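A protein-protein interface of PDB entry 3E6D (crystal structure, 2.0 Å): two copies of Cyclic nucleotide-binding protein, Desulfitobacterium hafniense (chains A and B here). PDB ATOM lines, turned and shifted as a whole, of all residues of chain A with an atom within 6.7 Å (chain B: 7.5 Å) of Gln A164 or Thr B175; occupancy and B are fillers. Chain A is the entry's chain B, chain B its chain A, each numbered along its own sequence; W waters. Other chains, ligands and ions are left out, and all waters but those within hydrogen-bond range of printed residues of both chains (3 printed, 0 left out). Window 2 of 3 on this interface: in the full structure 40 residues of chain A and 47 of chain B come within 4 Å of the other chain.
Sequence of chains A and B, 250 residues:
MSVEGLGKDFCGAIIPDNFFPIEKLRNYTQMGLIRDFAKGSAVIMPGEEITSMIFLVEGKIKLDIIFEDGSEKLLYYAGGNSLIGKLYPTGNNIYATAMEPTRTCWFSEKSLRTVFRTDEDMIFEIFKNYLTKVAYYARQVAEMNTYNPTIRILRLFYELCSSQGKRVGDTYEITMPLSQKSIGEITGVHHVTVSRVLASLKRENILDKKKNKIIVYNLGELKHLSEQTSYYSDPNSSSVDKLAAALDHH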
ATOM      1  N   TYR A 158       2.515 -13.715 -13.240  1.00  0.00           N
ATOM      2  CA  TYR A 158       2.037 -13.271 -11.936  1.00  0.00           C
ATOM      3  C   TYR A 158       1.848 -14.437 -10.987  1.00  0.00           C
ATOM      4  O   TYR A 158       2.230 -14.366  -9.821  1.00  0.00           O
ATOM      5  CB  TYR A 158       0.738 -12.468 -12.027  1.00  0.00           C
ATOM      6  CG  TYR A 158       0.236 -12.106 -10.646  1.00  0.00           C
ATOM      7  CD1 TYR A 158       0.940 -11.218  -9.844  1.00  0.00           C
ATOM      8  CD2 TYR A 158      -0.909 -12.695 -10.124  1.00  0.00           C
ATOM      9  CE1 TYR A 158       0.505 -10.906  -8.567  1.00  0.00           C
ATOM     10  CE2 TYR A 158      -1.354 -12.388  -8.849  1.00  0.00           C
ATOM     11  CZ  TYR A 158      -0.643 -11.495  -8.076  1.00  0.00           C
ATOM     12  OH  TYR A 158      -1.087 -11.192  -6.812  1.00  0.00           O
ATOM     13  N   GLU A 159       1.253 -15.509 -11.497  1.00  0.00           N
ATOM     14  CA  GLU A 159       1.019 -16.708 -10.709  1.00  0.00           C
ATOM     15  C   GLU A 159       2.348 -17.254 -10.203  1.00  0.00           C
ATOM     16  O   GLU A 159       2.493 -17.583  -9.025  1.00  0.00           O
ATOM     17  CB  GLU A 159       0.322 -17.760 -11.568  1.00  0.00           C
ATOM     18  CG  GLU A 159      -0.375 -18.836 -10.772  1.00  0.00           C
ATOM     19  CD  GLU A 159      -1.632 -18.327 -10.081  1.00  0.00           C
ATOM     20  OE1 GLU A 159      -2.090 -17.201 -10.393  1.00  0.00           O
ATOM     21  OE2 GLU A 159      -2.153 -19.061  -9.216  1.00  0.00           O
ATOM     22  N   LEU A 160       3.311 -17.354 -11.115  1.00  0.00           N
ATOM     23  CA  LEU A 160       4.654 -17.820 -10.796  1.00  0.00           C
ATOM     24  C   LEU A 160       5.316 -16.944  -9.741  1.00  0.00           C
ATOM     25  O   LEU A 160       5.921 -17.446  -8.798  1.00  0.00           O
ATOM     26  CB  LEU A 160       5.516 -17.842 -12.057  1.00  0.00           C
ATOM     27  CG  LEU A 160       5.935 -19.164 -12.711  1.00  0.00           C
ATOM     28  CD1 LEU A 160       5.114 -20.358 -12.253  1.00  0.00           C
ATOM     29  CD2 LEU A 160       5.933 -19.041 -14.238  1.00  0.00           C
ATOM     30  N   CYS A 161       5.192 -15.631  -9.895  1.00  0.00           N
ATOM     31  CA  CYS A 161       5.862 -14.719  -8.981  1.00  0.00           C
ATOM     32  C   CYS A 161       5.286 -14.764  -7.562  1.00  0.00           C
ATOM     33  O   CYS A 161       6.027 -14.908  -6.590  1.00  0.00           O
ATOM     34  CB  CYS A 161       5.845 -13.295  -9.534  1.00  0.00           C
ATOM     35  SG  CYS A 161       6.967 -12.167  -8.683  1.00  0.00           S
ATOM     36  N   SER A 162       3.969 -14.650  -7.435  1.00  0.00           N
ATOM     37  CA  SER A 162       3.357 -14.592  -6.110  1.00  0.00           C
ATOM     38  C   SER A 162       3.526 -15.924  -5.386  1.00  0.00           C
ATOM     39  O   SER A 162       3.557 -15.978  -4.158  1.00  0.00           O
ATOM     40  CB  SER A 162       1.876 -14.223  -6.195  1.00  0.00           C
ATOM     41  OG  SER A 162       1.129 -15.274  -6.768  1.00  0.00           O
ATOM     42  N   SER A 163       3.642 -16.995  -6.160  1.00  0.00           N
ATOM     43  CA  SER A 163       3.781 -18.328  -5.597  1.00  0.00           C
ATOM     44  C   SER A 163       5.241 -18.736  -5.369  1.00  0.00           C
ATOM     45  O   SER A 163       5.581 -19.248  -4.302  1.00  0.00           O
ATOM     46  CB  SER A 163       3.083 -19.349  -6.500  1.00  0.00           C
ATOM     47  OG  SER A 163       3.086 -20.628  -5.900  1.00  0.00           O
ATOM     48  N   GLN A 164       6.097 -18.504  -6.363  1.00  0.00           N
ATOM     49  CA  GLN A 164       7.471 -19.012  -6.333  1.00  0.00           C
ATOM     50  C   GLN A 164       8.550 -17.919  -6.272  1.00  0.00           C
ATOM     51  O   GLN A 164       9.738 -18.219  -6.132  1.00  0.00           O
ATOM     52  CB  GLN A 164       7.731 -19.920  -7.543  1.00  0.00           C
ATOM     53  CG  GLN A 164       6.677 -21.004  -7.746  1.00  0.00           C
ATOM     54  CD  GLN A 164       6.505 -21.870  -6.521  1.00  0.00           C
ATOM     55  OE1 GLN A 164       7.438 -22.539  -6.087  1.00  0.00           O
ATOM     56  NE2 GLN A 164       5.307 -21.860  -5.952  1.00  0.00           N
ATOM     57  N   GLY A 165       8.140 -16.659  -6.379  1.00  0.00           N
ATOM     58  CA  GLY A 165       9.088 -15.557  -6.389  1.00  0.00           C
ATOM     59  C   GLY A 165       9.764 -15.311  -5.047  1.00  0.00           C
ATOM     60  O   GLY A 165       9.107 -15.255  -4.008  1.00  0.00           O
ATOM     61  N   LYS A 166      11.084 -15.162  -5.067  1.00  0.00           N
ATOM     62  CA  LYS A 166      11.836 -14.819  -3.856  1.00  0.00           C
ATOM     63  C   LYS A 166      12.253 -13.346  -3.879  1.00  0.00           C
ATOM     64  O   LYS A 166      12.665 -12.824  -4.917  1.00  0.00           O
ATOM     65  CB  LYS A 166      13.071 -15.718  -3.715  1.00  0.00           C
ATOM     66  CG  LYS A 166      12.753 -17.205  -3.579  1.00  0.00           C
ATOM     67  CD  LYS A 166      14.026 -18.024  -3.380  1.00  0.00           C
ATOM     68  CE  LYS A 166      13.722 -19.494  -3.071  1.00  0.00           C
ATOM     69  NZ  LYS A 166      13.210 -20.231  -4.258  1.00  0.00           N
ATOM     70  N   GLU A 173      12.656 -12.798  -7.722  1.00  0.00           N
ATOM     71  CA  GLU A 173      13.329 -13.719  -8.620  1.00  0.00           C
ATOM     72  C   GLU A 173      12.634 -15.067  -8.592  1.00  0.00           C
ATOM     73  O   GLU A 173      12.417 -15.639  -7.523  1.00  0.00           O
ATOM     74  CB  GLU A 173      14.783 -13.915  -8.204  1.00  0.00           C
ATOM     75  CG  GLU A 173      15.652 -12.698  -8.401  1.00  0.00           C
ATOM     76  CD  GLU A 173      17.115 -12.992  -8.133  1.00  0.00           C
ATOM     77  OE1 GLU A 173      17.431 -14.111  -7.671  1.00  0.00           O
ATOM     78  OE2 GLU A 173      17.946 -12.098  -8.387  1.00  0.00           O
ATOM     79  N   ILE A 174      12.288 -15.565  -9.772  1.00  0.00           N
ATOM     80  CA  ILE A 174      11.757 -16.909  -9.913  1.00  0.00           C
ATOM     81  C   ILE A 174      12.854 -17.779 -10.518  1.00  0.00           C
ATOM     82  O   ILE A 174      13.337 -17.502 -11.610  1.00  0.00           O
ATOM     83  CB  ILE A 174      10.508 -16.921 -10.819  1.00  0.00           C
ATOM     84  CG1 ILE A 174       9.510 -15.854 -10.360  1.00  0.00           C
ATOM     85  CG2 ILE A 174       9.852 -18.307 -10.830  1.00  0.00           C
ATOM     86  CD1 ILE A 174       8.503 -15.467 -11.430  1.00  0.00           C
ATOM     87  N   THR A 175      13.268 -18.811  -9.793  1.00  0.00           N
ATOM     88  CA  THR A 175      14.294 -19.718 -10.297  1.00  0.00           C
ATOM     89  C   THR A 175      13.641 -20.833 -11.101  1.00  0.00           C
ATOM     90  O   THR A 175      12.945 -21.688 -10.552  1.00  0.00           O
ATOM     91  CB  THR A 175      15.141 -20.312  -9.163  1.00  0.00           C
ATOM     92  OG1 THR A 175      15.823 -19.253  -8.482  1.00  0.00           O
ATOM     93  CG2 THR A 175      16.164 -21.289  -9.719  1.00  0.00           C
ATOM     94  N   MET A 176      13.870 -20.813 -12.407  1.00  0.00           N
ATOM     95  CA  MET A 176      13.105 -21.645 -13.318  1.00  0.00           C
ATOM     96  C   MET A 176      13.566 -21.413 -14.747  1.00  0.00           C
ATOM     97  O   MET A 176      13.612 -20.273 -15.203  1.00  0.00           O
ATOM     98  CB  MET A 176      11.623 -21.289 -13.189  1.00  0.00           C
ATOM     99  CG  MET A 176      10.703 -22.003 -14.146  1.00  0.00           C
ATOM    100  SD  MET A 176       8.976 -21.736 -13.701  1.00  0.00           S
ATOM    101  CE  MET A 176       8.206 -23.044 -14.654  1.00  0.00           C
ATOM    102  N   LEU B 160       6.003 -26.946 -13.972  1.00  0.00           N
ATOM    103  CA  LEU B 160       5.956 -26.666 -12.539  1.00  0.00           C
ATOM    104  C   LEU B 160       6.639 -27.761 -11.727  1.00  0.00           C
ATOM    105  O   LEU B 160       7.364 -27.481 -10.777  1.00  0.00           O
ATOM    106  CB  LEU B 160       4.509 -26.521 -12.060  1.00  0.00           C
ATOM    107  CG  LEU B 160       3.951 -25.138 -11.737  1.00  0.00           C
ATOM    108  CD1 LEU B 160       4.474 -24.080 -12.694  1.00  0.00           C
ATOM    109  CD2 LEU B 160       2.425 -25.176 -11.736  1.00  0.00           C
ATOM    110  N   SER B 163      10.683 -28.029 -12.146  1.00  0.00           N
ATOM    111  CA  SER B 163      11.461 -26.894 -11.649  1.00  0.00           C
ATOM    112  C   SER B 163      11.163 -26.554 -10.188  1.00  0.00           C
ATOM    113  O   SER B 163      12.032 -26.061  -9.466  1.00  0.00           O
ATOM    114  CB  SER B 163      11.246 -25.660 -12.534  1.00  0.00           C
ATOM    115  OG  SER B 163       9.916 -25.170 -12.436  1.00  0.00           O
ATOM    116  N   GLN B 164       9.937 -26.833  -9.761  1.00  0.00           N
ATOM    117  CA  GLN B 164       9.467 -26.439  -8.438  1.00  0.00           C
ATOM    118  C   GLN B 164       9.301 -27.632  -7.500  1.00  0.00           C
ATOM    119  O   GLN B 164       9.207 -27.469  -6.285  1.00  0.00           O
ATOM    120  CB  GLN B 164       8.129 -25.702  -8.561  1.00  0.00           C
ATOM    121  CG  GLN B 164       8.196 -24.185  -8.435  1.00  0.00           C
ATOM    122  CD  GLN B 164       9.500 -23.600  -8.929  1.00  0.00           C
ATOM    123  OE1 GLN B 164      10.325 -23.155  -8.133  1.00  0.00           O
ATOM    124  NE2 GLN B 164       9.699 -23.603 -10.242  1.00  0.00           N
ATOM    125  N   GLY B 165       9.274 -28.834  -8.063  1.00  0.00           N
ATOM    126  CA  GLY B 165       8.894 -30.009  -7.303  1.00  0.00           C
ATOM    127  C   GLY B 165      10.009 -30.670  -6.517  1.00  0.00           C
ATOM    128  O   GLY B 165      11.152 -30.727  -6.967  1.00  0.00           O
ATOM    129  N   LYS B 166       9.664 -31.179  -5.338  1.00  0.00           N
ATOM    130  CA  LYS B 166      10.615 -31.892  -4.495  1.00  0.00           C
ATOM    131  C   LYS B 166      10.288 -33.380  -4.401  1.00  0.00           C
ATOM    132  O   LYS B 166       9.179 -33.767  -4.017  1.00  0.00           O
ATOM    133  CB  LYS B 166      10.670 -31.258  -3.108  1.00  0.00           C
ATOM    134  CG  LYS B 166      11.216 -29.839  -3.143  1.00  0.00           C
ATOM    135  CD  LYS B 166      11.158 -29.158  -1.796  1.00  0.00           C
ATOM    136  CE  LYS B 166      11.793 -27.776  -1.867  1.00  0.00           C
ATOM    137  NZ  LYS B 166      11.867 -27.133  -0.516  1.00  0.00           N
ATOM    138  N   GLU B 173       6.382 -33.392  -4.826  1.00  0.00           N
ATOM    139  CA  GLU B 173       5.459 -32.444  -4.211  1.00  0.00           C
ATOM    140  C   GLU B 173       5.814 -31.018  -4.569  1.00  0.00           C
ATOM    141  O   GLU B 173       6.979 -30.627  -4.533  1.00  0.00           O
ATOM    142  CB  GLU B 173       5.423 -32.608  -2.690  1.00  0.00           C
ATOM    143  CG  GLU B 173       4.726 -33.872  -2.228  1.00  0.00           C
ATOM    144  CD  GLU B 173       4.557 -33.934  -0.723  1.00  0.00           C
ATOM    145  OE1 GLU B 173       4.449 -32.864  -0.082  1.00  0.00           O
ATOM    146  OE2 GLU B 173       4.526 -35.059  -0.183  1.00  0.00           O
ATOM    147  N   ILE B 174       4.792 -30.251  -4.928  1.00  0.00           N
ATOM    148  CA  ILE B 174       4.937 -28.842  -5.230  1.00  0.00           C
ATOM    149  C   ILE B 174       4.039 -28.066  -4.281  1.00  0.00           C
ATOM    150  O   ILE B 174       2.823 -28.272  -4.263  1.00  0.00           O
ATOM    151  CB  ILE B 174       4.492 -28.525  -6.671  1.00  0.00           C
ATOM    152  CG1 ILE B 174       5.123 -29.508  -7.665  1.00  0.00           C
ATOM    153  CG2 ILE B 174       4.833 -27.086  -7.022  1.00  0.00           C
ATOM    154  CD1 ILE B 174       4.398 -29.589  -9.007  1.00  0.00           C
ATOM    155  N   THR B 175       4.632 -27.182  -3.488  1.00  0.00           N
ATOM    156  CA  THR B 175       3.850 -26.369  -2.570  1.00  0.00           C
ATOM    157  C   THR B 175       3.512 -25.044  -3.213  1.00  0.00           C
ATOM    158  O   THR B 175       4.384 -24.205  -3.442  1.00  0.00           O
ATOM    159  CB  THR B 175       4.572 -26.119  -1.243  1.00  0.00           C
ATOM    160  OG1 THR B 175       5.042 -27.363  -0.715  1.00  0.00           O
ATOM    161  CG2 THR B 175       3.615 -25.477  -0.245  1.00  0.00           C
ATOM    162  N   MET B 176       2.231 -24.873  -3.506  1.00  0.00           N
ATOM    163  CA  MET B 176       1.732 -23.672  -4.145  1.00  0.00           C
ATOM    164  C   MET B 176       0.246 -23.856  -4.380  1.00  0.00           C
ATOM    165  O   MET B 176      -0.205 -24.961  -4.691  1.00  0.00           O
ATOM    166  CB  MET B 176       2.427 -23.454  -5.487  1.00  0.00           C
ATOM    167  CG  MET B 176       1.885 -24.334  -6.607  1.00  0.00           C
ATOM    168  SD  MET B 176       2.791 -24.157  -8.159  1.00  0.00           S
ATOM    169  CE  MET B 176       2.068 -22.669  -8.861  1.00  0.00           C
ATOM    170  N   PRO B 177      -0.531 -22.780  -4.212  1.00  0.00           N
ATOM    171  CA  PRO B 177      -1.928 -22.872  -4.623  1.00  0.00           C
ATOM    172  C   PRO B 177      -1.974 -22.733  -6.129  1.00  0.00           C
ATOM    173  O   PRO B 177      -0.994 -22.278  -6.718  1.00  0.00           O
ATOM    174  CB  PRO B 177      -2.573 -21.655  -3.961  1.00  0.00           C
ATOM    175  CG  PRO B 177      -1.463 -20.680  -3.774  1.00  0.00           C
ATOM    176  CD  PRO B 177      -0.177 -21.451  -3.678  1.00  0.00           C
ATOM    177  N   ASN B 212      -3.486 -26.609  -1.023  1.00  0.00           N
ATOM    178  CA  ASN B 212      -2.378 -25.872  -1.629  1.00  0.00           C
ATOM    179  C   ASN B 212      -1.136 -26.730  -1.877  1.00  0.00           C
ATOM    180  O   ASN B 212      -0.010 -26.239  -1.849  1.00  0.00           O
ATOM    181  CB  ASN B 212      -2.013 -24.653  -0.779  1.00  0.00           C
ATOM    182  CG  ASN B 212      -3.097 -23.601  -0.783  1.00  0.00           C
ATOM    183  OD1 ASN B 212      -3.821 -23.445  -1.762  1.00  0.00           O
ATOM    184  ND2 ASN B 212      -3.218 -22.871   0.318  1.00  0.00           N
ATOM    185  N   LYS B 213      -1.346 -28.014  -2.120  1.00  0.00           N
ATOM    186  CA  LYS B 213      -0.240 -28.917  -2.385  1.00  0.00           C
ATOM    187  C   LYS B 213      -0.544 -29.763  -3.613  1.00  0.00           C
ATOM    188  O   LYS B 213      -1.609 -30.379  -3.714  1.00  0.00           O
ATOM    189  CB  LYS B 213       0.030 -29.803  -1.163  1.00  0.00           C
ATOM    190  CG  LYS B 213       1.300 -30.630  -1.261  1.00  0.00           C
ATOM    191  CD  LYS B 213       1.749 -31.135   0.104  1.00  0.00           C
ATOM    192  N   ILE B 214       0.390 -29.779  -4.555  1.00  0.00           N
ATOM    193  CA  ILE B 214       0.257 -30.619  -5.734  1.00  0.00           C
ATOM    194  C   ILE B 214       1.166 -31.834  -5.620  1.00  0.00           C
ATOM    195  O   ILE B 214       2.375 -31.707  -5.420  1.00  0.00           O
ATOM    196  CB  ILE B 214       0.602 -29.858  -7.024  1.00  0.00           C
ATOM    197  CG1 ILE B 214      -0.282 -28.617  -7.168  1.00  0.00           C
ATOM    198  CG2 ILE B 214       0.449 -30.775  -8.228  1.00  0.00           C
ATOM    199  CD1 ILE B 214       0.037 -27.778  -8.384  1.00  0.00           C
ATOM    200  N   ILE B 215       0.576 -33.017  -5.752  1.00  0.00           N
ATOM    201  CA  ILE B 215       1.333 -34.251  -5.653  1.00  0.00           C
ATOM    202  C   ILE B 215       1.340 -34.960  -6.994  1.00  0.00           C
ATOM    203  O   ILE B 215       0.282 -35.292  -7.528  1.00  0.00           O
ATOM    204  CB  ILE B 215       0.730 -35.195  -4.608  1.00  0.00           C
ATOM    205  CG1 ILE B 215       0.447 -34.449  -3.306  1.00  0.00           C
ATOM    206  CG2 ILE B 215       1.654 -36.382  -4.366  1.00  0.00           C
ATOM    207  CD1 ILE B 215      -0.441 -35.228  -2.356  1.00  0.00           C
HETATM  208  O   HOH W   1       6.959 -24.417  -3.635  1.00  0.00           O
HETATM  209  O   HOH W   2      11.788 -21.916  -6.559  1.00  0.00           O
HETATM  210  O   HOH W   3      13.852 -24.045  -9.152  1.00  0.00           O
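Leu B160 touches its own counterpart, Leu A160.
Ser A163 touches Met B176, and with the chains exchanged Met A176 touches Ser B163.
Gln A164 touches Thr B175, and with the chains exchanged Thr A175 touches Gln B164.
Gln A164 touches Met B176, and with the chains exchanged Met A176 touches Gln B164.
Water W2 lies within hydrogen-bond range of OE1 of Gln B164 (2.5 Å) and NZ of Lys A166 (3.2 Å).
Water W1 bridges the backbone carbonyl oxygen (O) of Thr B175 (2.6 Å) and the side-chain amide oxygen (OE1) of Gln A164 (3.1 Å).
Water W3 lies within hydrogen-bond range of the backbone carbonyl oxygen of Ser B163 (2.7 Å) and the backbone carbonyl oxygen of Thr A175 (2.9 Å).
SD of Met A176 sits close to OG of Ser B163, at 3.8 Å.
The side-chain amide nitrogen (NE2) of Gln A164 is in hydrogen-bond range of the side-chain hydroxyl (OG) of Ser A163 (2.5 Å).
The backbone carbonyl oxygen (O) of Asn B212 is in hydrogen-bond range of the backbone NH (N) of Met B176 (3.1 Å).
O of Leu A160 lies within hydrogen-bond range of N of Gly A165, at 3.4 Å.
OG of Ser B163 sits at hydrogen-bond distance from NE2 of Gln B164.
Printed residues of chain A that touch a printed residue of chain B: Leu A160, Ser A163, Gln A164, Thr A175 and Met A176.
Hydrophobic or aromatic side chains of chain A that line the printed part of chain B: Leu A160 and Met A176.
Of the 14 printed residues of chain B, 5 touch a printed residue of chain A.
Printed residues of chain B that touch a printed residue of chain A: Leu B160, Ser B163, Gln B164, Thr B175 and Met B176.
Hydrophobic or aromatic side chains of chain B within 4 Å of the printed part of chain A: Leu B160 and Met B176.
Among the printed residues, 8 pairs touch across the chains.
Among the printed residues, no Asp or Glu carboxylate lies within 4 Å of a Lys or Arg side-chain nitrogen of the other chain.
Among the printed residues, merely in contact across the chains: Leu A160 with Leu B160, Ser A163 with Met B176, Gln A164 with Gln B164, Gln A164 with Thr B175, Gln A164 with Met B176, Thr A175 with Gln B164 and Met A176 with Gln B164.
Of chain B, only Gln B164, Thr B175 and Met B176 come within 4 Å of Gln A164.
Of chain A, only Gln A164 (3.6 Å) comes within 4 Å of Thr B175.
Of chain B, only Met B176 (2.9 Å) comes within 4 Å of Ser A163.
Of the printed residues of chain A, Gln B164 touches Gln A164 (3.0 Å), Thr A175 (3.8 Å) and Met A176 (3.997 Å).
Of the printed residues of chain A, Leu B160 touches Leu A160.
Ile B214 touches none of the printed residues of chain A.
The nearest residue of chain B that does not touch Gln A164 is Ile B174 (5.3 Å).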
